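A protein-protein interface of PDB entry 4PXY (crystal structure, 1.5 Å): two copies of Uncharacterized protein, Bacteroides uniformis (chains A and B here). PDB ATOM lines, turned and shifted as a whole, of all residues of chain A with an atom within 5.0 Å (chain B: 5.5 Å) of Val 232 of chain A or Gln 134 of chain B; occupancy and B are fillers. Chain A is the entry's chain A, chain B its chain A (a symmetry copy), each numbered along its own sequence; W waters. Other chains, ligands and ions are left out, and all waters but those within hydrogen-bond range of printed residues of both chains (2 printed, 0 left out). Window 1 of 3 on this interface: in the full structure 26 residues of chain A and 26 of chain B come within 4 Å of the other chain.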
ATOM      1  N   PHE A  41     -19.197  -6.550 -31.615  1.00  0.00           N
ATOM      2  CA  PHE A  41     -19.264  -6.569 -30.171  1.00  0.00           C
ATOM      3  C   PHE A  41     -20.260  -7.647 -29.692  1.00  0.00           C
ATOM      4  O   PHE A  41     -19.940  -8.461 -28.832  1.00  0.00           O
ATOM      5  CB  PHE A  41     -19.613  -5.154 -29.675  1.00  0.00           C
ATOM      6  CG  PHE A  41     -19.944  -5.038 -28.222  1.00  0.00           C
ATOM      7  CD1 PHE A  41     -18.944  -4.845 -27.277  1.00  0.00           C
ATOM      8  CD2 PHE A  41     -21.270  -5.000 -27.823  1.00  0.00           C
ATOM      9  CE1 PHE A  41     -19.295  -4.644 -25.952  1.00  0.00           C
ATOM     10  CE2 PHE A  41     -21.614  -4.803 -26.510  1.00  0.00           C
ATOM     11  CZ  PHE A  41     -20.604  -4.654 -25.601  1.00  0.00           C
ATOM     12  N   LEU A  45     -19.876 -11.344 -27.803  1.00  0.00           N
ATOM     13  CA  LEU A  45     -20.658 -11.731 -26.616  1.00  0.00           C
ATOM     14  C   LEU A  45     -21.309 -13.086 -26.808  1.00  0.00           C
ATOM     15  O   LEU A  45     -21.606 -13.773 -25.820  1.00  0.00           O
ATOM     16  CB  LEU A  45     -21.702 -10.670 -26.241  1.00  0.00           C
ATOM     17  CG  LEU A  45     -21.206  -9.364 -25.722  1.00  0.00           C
ATOM     18  CD1 LEU A  45     -22.362  -8.452 -25.442  1.00  0.00           C
ATOM     19  CD2 LEU A  45     -20.325  -9.501 -24.466  1.00  0.00           C
ATOM     20  N   ASN A 228     -17.942   0.323 -22.832  1.00  0.00           N
ATOM     21  CA  ASN A 228     -18.216  -1.044 -23.239  1.00  0.00           C
ATOM     22  C   ASN A 228     -19.033  -1.786 -22.189  1.00  0.00           C
ATOM     23  O   ASN A 228     -19.969  -2.534 -22.533  1.00  0.00           O
ATOM     24  CB  ASN A 228     -16.932  -1.792 -23.574  1.00  0.00           C
ATOM     25  CG  ASN A 228     -16.163  -1.148 -24.746  1.00  0.00           C
ATOM     26  OD1 ASN A 228     -16.695  -0.276 -25.433  1.00  0.00           O
ATOM     27  ND2 ASN A 228     -14.952  -1.601 -25.000  1.00  0.00           N
ATOM     28  N   LEU A 229     -18.755  -1.533 -20.917  1.00  0.00           N
ATOM     29  CA  LEU A 229     -19.482  -2.162 -19.819  1.00  0.00           C
ATOM     30  C   LEU A 229     -20.915  -1.667 -19.726  1.00  0.00           C
ATOM     31  O   LEU A 229     -21.839  -2.467 -19.520  1.00  0.00           O
ATOM     32  CB  LEU A 229     -18.752  -1.932 -18.486  1.00  0.00           C
ATOM     33  CG  LEU A 229     -19.363  -2.619 -17.267  1.00  0.00           C
ATOM     34  CD1 LEU A 229     -19.658  -4.073 -17.531  1.00  0.00           C
ATOM     35  CD2 LEU A 229     -18.414  -2.441 -16.076  1.00  0.00           C
ATOM     36  N   LEU A 230     -21.117  -0.367 -19.962  1.00  0.00           N
ATOM     37  CA  LEU A 230     -22.473   0.185 -20.068  1.00  0.00           C
ATOM     38  C   LEU A 230     -23.292  -0.586 -21.117  1.00  0.00           C
ATOM     39  O   LEU A 230     -24.438  -0.921 -20.859  1.00  0.00           O
ATOM     40  CB  LEU A 230     -22.394   1.656 -20.418  1.00  0.00           C
ATOM     41  CG  LEU A 230     -23.722   2.312 -20.813  1.00  0.00           C
ATOM     42  CD1 LEU A 230     -24.647   2.400 -19.621  1.00  0.00           C
ATOM     43  CD2 LEU A 230     -23.392   3.681 -21.368  1.00  0.00           C
ATOM     44  N   LEU A 231     -22.713  -0.858 -22.276  1.00  0.00           N
ATOM     45  CA  LEU A 231     -23.421  -1.597 -23.309  1.00  0.00           C
ATOM     46  C   LEU A 231     -23.750  -3.013 -22.910  1.00  0.00           C
ATOM     47  O   LEU A 231     -24.881  -3.476 -23.143  1.00  0.00           O
ATOM     48  CB  LEU A 231     -22.684  -1.552 -24.657  1.00  0.00           C
ATOM     49  CG  LEU A 231     -23.006  -0.347 -25.524  1.00  0.00           C
ATOM     50  CD1 LEU A 231     -22.634   1.001 -24.936  1.00  0.00           C
ATOM     51  CD2 LEU A 231     -22.378  -0.484 -26.887  1.00  0.00           C
ATOM     52  N   VAL A 232     -22.779  -3.743 -22.351  1.00  0.00           N
ATOM     53  CA  VAL A 232     -23.054  -5.063 -21.856  1.00  0.00           C
ATOM     54  C   VAL A 232     -24.254  -5.002 -20.887  1.00  0.00           C
ATOM     55  O   VAL A 232     -25.169  -5.815 -20.946  1.00  0.00           O
ATOM     56  CB  VAL A 232     -21.831  -5.654 -21.170  1.00  0.00           C
ATOM     57  CG1 VAL A 232     -22.193  -6.974 -20.568  1.00  0.00           C
ATOM     58  CG2 VAL A 232     -20.692  -5.866 -22.147  1.00  0.00           C
ATOM     59  N   ASN A 233     -24.176  -4.096 -19.932  1.00  0.00           N
ATOM     60  CA  ASN A 233     -25.159  -3.998 -18.864  1.00  0.00           C
ATOM     61  C   ASN A 233     -26.546  -3.660 -19.409  1.00  0.00           C
ATOM     62  O   ASN A 233     -27.560  -4.159 -18.899  1.00  0.00           O
ATOM     63  CB  ASN A 233     -24.793  -2.907 -17.851  1.00  0.00           C
ATOM     64  CG  ASN A 233     -23.581  -3.215 -17.028  1.00  0.00           C
ATOM     65  OD1 ASN A 233     -23.097  -4.375 -16.982  1.00  0.00           O
ATOM     66  ND2 ASN A 233     -23.121  -2.183 -16.333  1.00  0.00           N
ATOM     67  N   ALA A 234     -26.612  -2.782 -20.405  1.00  0.00           N
ATOM     68  CA  ALA A 234     -27.873  -2.372 -21.001  1.00  0.00           C
ATOM     69  C   ALA A 234     -28.591  -3.561 -21.656  1.00  0.00           C
ATOM     70  O   ALA A 234     -29.775  -3.827 -21.471  1.00  0.00           O
ATOM     71  CB  ALA A 234     -27.642  -1.260 -22.008  1.00  0.00           C
ATOM     72  N   PHE A 235     -27.828  -4.312 -22.429  1.00  0.00           N
ATOM     73  CA  PHE A 235     -28.295  -5.506 -23.117  1.00  0.00           C
ATOM     74  C   PHE A 235     -28.721  -6.535 -22.069  1.00  0.00           C
ATOM     75  O   PHE A 235     -29.839  -7.067 -22.131  1.00  0.00           O
ATOM     76  CB  PHE A 235     -27.125  -6.053 -23.936  1.00  0.00           C
ATOM     77  CG  PHE A 235     -27.322  -7.427 -24.538  1.00  0.00           C
ATOM     78  CD1 PHE A 235     -28.337  -7.676 -25.440  1.00  0.00           C
ATOM     79  CD2 PHE A 235     -26.405  -8.405 -24.308  1.00  0.00           C
ATOM     80  CE1 PHE A 235     -28.487  -8.920 -26.007  1.00  0.00           C
ATOM     81  CE2 PHE A 235     -26.512  -9.651 -24.946  1.00  0.00           C
ATOM     82  CZ  PHE A 235     -27.592  -9.875 -25.795  1.00  0.00           C
ATOM     83  N   ARG A 236     -27.884  -6.799 -21.089  1.00  0.00           N
ATOM     84  CA  ARG A 236     -28.189  -7.830 -20.094  1.00  0.00           C
ATOM     85  C   ARG A 236     -29.475  -7.490 -19.330  1.00  0.00           C
ATOM     86  O   ARG A 236     -30.325  -8.364 -19.071  1.00  0.00           O
ATOM     87  CB  ARG A 236     -27.027  -7.975 -19.142  1.00  0.00           C
ATOM     88  CG  ARG A 236     -27.142  -9.224 -18.299  1.00  0.00           C
ATOM     89  CD  ARG A 236     -26.063  -9.300 -17.210  1.00  0.00           C
ATOM     90  NE  ARG A 236     -25.986 -10.620 -16.619  1.00  0.00           N
ATOM     91  CZ  ARG A 236     -26.890 -11.181 -15.793  1.00  0.00           C
ATOM     92  NH1 ARG A 236     -27.895 -10.442 -15.341  1.00  0.00           N
ATOM     93  NH2 ARG A 236     -26.745 -12.433 -15.400  1.00  0.00           N
ATOM     94  N   TRP A 237     -29.627  -6.225 -18.964  1.00  0.00           N
ATOM     95  CA  TRP A 237     -30.784  -5.796 -18.181  1.00  0.00           C
ATOM     96  C   TRP A 237     -32.070  -6.008 -18.952  1.00  0.00           C
ATOM     97  O   TRP A 237     -33.013  -6.652 -18.436  1.00  0.00           O
ATOM     98  CB  TRP A 237     -30.640  -4.335 -17.770  1.00  0.00           C
ATOM     99  CG  TRP A 237     -31.814  -3.799 -16.985  1.00  0.00           C
ATOM    100  CD1 TRP A 237     -32.234  -4.235 -15.770  1.00  0.00           C
ATOM    101  CD2 TRP A 237     -32.687  -2.729 -17.357  1.00  0.00           C
ATOM    102  NE1 TRP A 237     -33.324  -3.491 -15.352  1.00  0.00           N
ATOM    103  CE2 TRP A 237     -33.599  -2.553 -16.311  1.00  0.00           C
ATOM    104  CE3 TRP A 237     -32.781  -1.895 -18.458  1.00  0.00           C
ATOM    105  CZ2 TRP A 237     -34.590  -1.564 -16.344  1.00  0.00           C
ATOM    106  CZ3 TRP A 237     -33.783  -0.925 -18.497  1.00  0.00           C
ATOM    107  CH2 TRP A 237     -34.680  -0.782 -17.423  1.00  0.00           C
ATOM    108  N   ASN B 130     -16.824 -16.588 -15.468  1.00  0.00           N
ATOM    109  CA  ASN B 130     -17.935 -16.056 -16.240  1.00  0.00           C
ATOM    110  C   ASN B 130     -17.650 -16.269 -17.713  1.00  0.00           C
ATOM    111  O   ASN B 130     -16.506 -16.413 -18.150  1.00  0.00           O
ATOM    112  CB  ASN B 130     -18.151 -14.573 -15.981  1.00  0.00           C
ATOM    113  CG  ASN B 130     -17.039 -13.733 -16.508  1.00  0.00           C
ATOM    114  OD1 ASN B 130     -15.902 -13.891 -16.061  1.00  0.00           O
ATOM    115  ND2 ASN B 130     -17.321 -12.872 -17.478  1.00  0.00           N
ATOM    116  N   PRO B 132     -19.542 -14.515 -21.545  1.00  0.00           N
ATOM    117  CA  PRO B 132     -18.339 -14.243 -22.313  1.00  0.00           C
ATOM    118  C   PRO B 132     -17.423 -13.239 -21.651  1.00  0.00           C
ATOM    119  O   PRO B 132     -17.776 -12.598 -20.677  1.00  0.00           O
ATOM    120  CB  PRO B 132     -18.917 -13.656 -23.640  1.00  0.00           C
ATOM    121  CG  PRO B 132     -20.107 -12.831 -23.128  1.00  0.00           C
ATOM    122  CD  PRO B 132     -20.708 -13.754 -22.074  1.00  0.00           C
ATOM    123  N   PRO B 133     -16.198 -13.074 -22.209  1.00  0.00           N
ATOM    124  CA  PRO B 133     -15.365 -11.988 -21.766  1.00  0.00           C
ATOM    125  C   PRO B 133     -16.109 -10.652 -21.802  1.00  0.00           C
ATOM    126  O   PRO B 133     -16.834 -10.348 -22.742  1.00  0.00           O
ATOM    127  CB  PRO B 133     -14.219 -12.008 -22.804  1.00  0.00           C
ATOM    128  CG  PRO B 133     -14.138 -13.399 -23.225  1.00  0.00           C
ATOM    129  CD  PRO B 133     -15.573 -13.888 -23.258  1.00  0.00           C
ATOM    130  N   GLN B 134     -15.918  -9.883 -20.750  1.00  0.00           N
ATOM    131  CA  GLN B 134     -16.532  -8.559 -20.656  1.00  0.00           C
ATOM    132  C   GLN B 134     -15.691  -7.722 -19.699  1.00  0.00           C
ATOM    133  O   GLN B 134     -14.988  -8.227 -18.806  1.00  0.00           O
ATOM    134  CB  GLN B 134     -17.976  -8.642 -20.162  1.00  0.00           C
ATOM    135  CG  GLN B 134     -18.097  -9.132 -18.703  1.00  0.00           C
ATOM    136  CD  GLN B 134     -19.467  -8.819 -18.149  1.00  0.00           C
ATOM    137  OE1 GLN B 134     -20.401  -9.573 -18.328  1.00  0.00           O
ATOM    138  NE2 GLN B 134     -19.607  -7.638 -17.561  1.00  0.00           N
ATOM    139  N   PRO B 135     -15.809  -6.412 -19.823  1.00  0.00           N
ATOM    140  CA  PRO B 135     -15.194  -5.518 -18.832  1.00  0.00           C
ATOM    141  C   PRO B 135     -15.897  -5.673 -17.485  1.00  0.00           C
ATOM    142  O   PRO B 135     -17.013  -6.135 -17.425  1.00  0.00           O
ATOM    143  CB  PRO B 135     -15.447  -4.102 -19.362  1.00  0.00           C
ATOM    144  CG  PRO B 135     -16.346  -4.268 -20.497  1.00  0.00           C
ATOM    145  CD  PRO B 135     -16.575  -5.673 -20.842  1.00  0.00           C
ATOM    146  N   VAL B 136     -15.210  -5.307 -16.435  1.00  0.00           N
ATOM    147  CA  VAL B 136     -15.713  -5.384 -15.074  1.00  0.00           C
ATOM    148  C   VAL B 136     -15.152  -4.277 -14.238  1.00  0.00           C
ATOM    149  O   VAL B 136     -14.039  -3.778 -14.501  1.00  0.00           O
ATOM    150  CB  VAL B 136     -15.403  -6.713 -14.392  1.00  0.00           C
ATOM    151  CG1 VAL B 136     -16.220  -7.871 -15.006  1.00  0.00           C
ATOM    152  CG2 VAL B 136     -13.910  -7.020 -14.435  1.00  0.00           C
ATOM    153  N   ALA B 157     -11.865  -2.435 -15.895  1.00  0.00           N
ATOM    154  CA  ALA B 157     -10.849  -3.101 -16.680  1.00  0.00           C
ATOM    155  C   ALA B 157     -11.484  -3.569 -17.964  1.00  0.00           C
ATOM    156  O   ALA B 157     -12.653  -3.965 -17.988  1.00  0.00           O
ATOM    157  CB  ALA B 157     -10.340  -4.319 -15.943  1.00  0.00           C
ATOM    158  N   PRO B 158     -10.737  -3.590 -19.070  1.00  0.00           N
ATOM    159  CA  PRO B 158     -11.273  -4.107 -20.326  1.00  0.00           C
ATOM    160  C   PRO B 158     -11.591  -5.586 -20.269  1.00  0.00           C
ATOM    161  O   PRO B 158     -11.294  -6.305 -19.300  1.00  0.00           O
ATOM    162  CB  PRO B 158     -10.163  -3.818 -21.340  1.00  0.00           C
ATOM    163  CG  PRO B 158      -9.066  -3.227 -20.622  1.00  0.00           C
ATOM    164  CD  PRO B 158      -9.382  -3.043 -19.193  1.00  0.00           C
ATOM    165  N   ALA B 159     -12.212  -6.065 -21.331  1.00  0.00           N
ATOM    166  CA  ALA B 159     -12.822  -7.367 -21.326  1.00  0.00           C
ATOM    167  C   ALA B 159     -11.824  -8.505 -21.131  1.00  0.00           C
ATOM    168  O   ALA B 159     -10.785  -8.553 -21.807  1.00  0.00           O
ATOM    169  CB  ALA B 159     -13.626  -7.586 -22.612  1.00  0.00           C
ATOM    170  N   SER B 160     -12.233  -9.449 -20.308  1.00  0.00           N
ATOM    171  CA  SER B 160     -11.596 -10.746 -20.161  1.00  0.00           C
ATOM    172  C   SER B 160     -12.681 -11.651 -19.605  1.00  0.00           C
ATOM    173  O   SER B 160     -13.732 -11.178 -19.074  1.00  0.00           O
ATOM    174  CB  SER B 160     -10.378 -10.640 -19.238  1.00  0.00           C
ATOM    175  OG  SER B 160      -9.652 -11.880 -19.207  1.00  0.00           O
ATOM    176  N   GLU B 161     -12.434 -12.963 -19.651  1.00  0.00           N
ATOM    177  CA  GLU B 161     -13.151 -13.863 -18.780  1.00  0.00           C
ATOM    178  C   GLU B 161     -12.324 -14.002 -17.519  1.00  0.00           C
ATOM    179  O   GLU B 161     -11.117 -13.788 -17.558  1.00  0.00           O
ATOM    180  CB  GLU B 161     -13.561 -15.231 -19.345  1.00  0.00           C
ATOM    181  CG  GLU B 161     -12.533 -16.356 -19.351  1.00  0.00           C
ATOM    182  CD  GLU B 161     -11.418 -16.188 -20.360  1.00  0.00           C
ATOM    183  OE1 GLU B 161     -11.078 -15.022 -20.728  1.00  0.00           O
ATOM    184  OE2 GLU B 161     -10.862 -17.240 -20.753  1.00  0.00           O
ATOM    185  N   TRP B 162     -13.018 -14.094 -16.402  1.00  0.00           N
ATOM    186  CA  TRP B 162     -12.444 -13.961 -15.084  1.00  0.00           C
ATOM    187  C   TRP B 162     -12.640 -15.240 -14.278  1.00  0.00           C
ATOM    188  O   TRP B 162     -13.680 -15.871 -14.373  1.00  0.00           O
ATOM    189  CB  TRP B 162     -13.071 -12.786 -14.371  1.00  0.00           C
ATOM    190  CG  TRP B 162     -12.982 -11.498 -15.163  1.00  0.00           C
ATOM    191  CD1 TRP B 162     -13.953 -10.957 -15.932  1.00  0.00           C
ATOM    192  CD2 TRP B 162     -11.877 -10.601 -15.229  1.00  0.00           C
ATOM    193  NE1 TRP B 162     -13.520  -9.780 -16.498  1.00  0.00           N
ATOM    194  CE2 TRP B 162     -12.240  -9.546 -16.105  1.00  0.00           C
ATOM    195  CE3 TRP B 162     -10.585 -10.625 -14.695  1.00  0.00           C
ATOM    196  CZ2 TRP B 162     -11.396  -8.524 -16.399  1.00  0.00           C
ATOM    197  CZ3 TRP B 162      -9.759  -9.561 -14.938  1.00  0.00           C
ATOM    198  CH2 TRP B 162     -10.153  -8.536 -15.811  1.00  0.00           C
ATOM    199  N   LEU B 188     -22.720 -11.801 -12.698  1.00  0.00           N
ATOM    200  CA  LEU B 188     -21.747 -11.569 -13.739  1.00  0.00           C
ATOM    201  C   LEU B 188     -21.781 -12.683 -14.784  1.00  0.00           C
ATOM    202  O   LEU B 188     -21.424 -13.827 -14.494  1.00  0.00           O
ATOM    203  CB  LEU B 188     -20.334 -11.518 -13.114  1.00  0.00           C
ATOM    204  CG  LEU B 188     -19.181 -11.375 -14.119  1.00  0.00           C
ATOM    205  CD1 LEU B 188     -19.275 -10.079 -14.930  1.00  0.00           C
ATOM    206  CD2 LEU B 188     -17.820 -11.481 -13.454  1.00  0.00           C
ATOM    207  N   GLY B 189     -22.155 -12.334 -16.006  1.00  0.00           N
ATOM    208  CA  GLY B 189     -22.134 -13.294 -17.078  1.00  0.00           C
ATOM    209  C   GLY B 189     -23.400 -13.305 -17.884  1.00  0.00           C
ATOM    210  O   GLY B 189     -24.500 -12.958 -17.419  1.00  0.00           O
ATOM    211  N   ILE B 190     -23.285 -13.742 -19.130  1.00  0.00           N
ATOM    212  CA  ILE B 190     -24.415 -13.907 -20.031  1.00  0.00           C
ATOM    213  C   ILE B 190     -24.628 -15.370 -20.384  1.00  0.00           C
ATOM    214  O   ILE B 190     -25.718 -15.896 -20.208  1.00  0.00           O
ATOM    215  CB  ILE B 190     -24.211 -13.053 -21.319  1.00  0.00           C
ATOM    216  CG1 ILE B 190     -24.154 -11.593 -20.911  1.00  0.00           C
ATOM    217  CG2 ILE B 190     -25.326 -13.304 -22.343  1.00  0.00           C
ATOM    218  CD1 ILE B 190     -23.826 -10.632 -22.016  1.00  0.00           C
HETATM  219  O   HOH W   1     -21.651  -6.239 -15.973  1.00  0.00           O
HETATM  220  O   HOH W   2     -22.779  -9.711 -16.958  1.00  0.00           O
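Water W1 bridges OD1 of Asn 233 of chain A (2.6 Å) and NE2 of Gln 134 of chain B (2.9 Å).
Water W2 lies within hydrogen-bond range of OE1 of Gln 134 of chain B, N of Gly 189 of chain B and NE of Arg 236 of chain A.
No position is printed for both chains.
Of the 7 pairs that touch across the chains among the printed residues, none has its exchanged pair printed and touching as well.
O of Leu 45 of chain A touches CG of Pro 132 of chain B, at 3.2 Å.
Leu 45 of chain A touches Pro 133 of chain B (CD2 to O, 3.98 Å).
Pro 135 of chain B touches Asn 228 of chain A (CG to CB, 3.99 Å).
Leu 229 of chain A touches Gln 134 of chain B.
Leu 229 of chain A touches Pro 135 of chain B (CD1 to O, 3.4 Å).
Gln 134 of chain B touches Val 232 of chain A.
Printed residues of chain B that touch a printed residue of chain A: Pro 132, Pro 133, Gln 134, Pro 135 and Gly 189.
Hydrophobic or aromatic side chains of chain B that line the printed part of chain A: Pro 132 and Pro 135.
Of the 12 printed residues of chain A, 5 touch a printed residue of chain B.
Hydrophobic or aromatic side chains of chain A within 4 Å of the printed part of chain B: Leu 45, Leu 229 and Val 232.
Among the printed residues, 7 pairs touch across the chains.
Among the printed residues, no Asp or Glu carboxylate lies within 4 Å of a Lys or Arg side-chain nitrogen of the other chain.
Printed residues of chain B within 4 Å of Leu 45 of chain A: Pro 132 and Pro 133.
Leu 231 of chain A touches none of the printed residues of chain B.
Val 232 of chain A touches just one residue of chain B: Gln 134 (3.9 Å).
Printed residues of chain B within 4 Å of Arg 236 of chain A: Gly 189 (2.9 Å).
Of the printed residues of chain A, Pro 133 of chain B touches Leu 45 (3.98 Å).
Of chain A, only Leu 229 and Val 232 come within 4 Å of Gln 134 of chain B.
Of the printed residues of chain A, Pro 135 of chain B touches Asn 228 (3.99 Å) and Leu 229 (3.4 Å).
Glu 161 of chain B touches none of the printed residues of chain A.
Printed residues of chain A within 4 Å of Gly 189 of chain B: Arg 236 (2.9 Å).
The nearest residue of chain A that does not touch Gln 134 of chain B is Asn 233 of chain A (4.8 Å).
The side-chain amide oxygen (OD1) of Asn 233 of chain A lies close to the backbone carbonyl oxygen (O) of Leu 229 of chain A (3.4 Å).
O of Pro 132 of chain B is in hydrogen-bond range of ND2 of Asn 130 of chain B.
N of Gln 134 of chain B sits at hydrogen-bond distance from O of Ser 160 of chain B (3.0 Å).
The backbone carbonyl oxygen (O) of Gln 134 of chain B lies within hydrogen-bond range of the indole nitrogen (NE1) of Trp 162 of chain B (3.1 Å).
O of Gly 189 of chain B is in hydrogen-bond range of NE of Arg 236 of chain A (2.9 Å).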
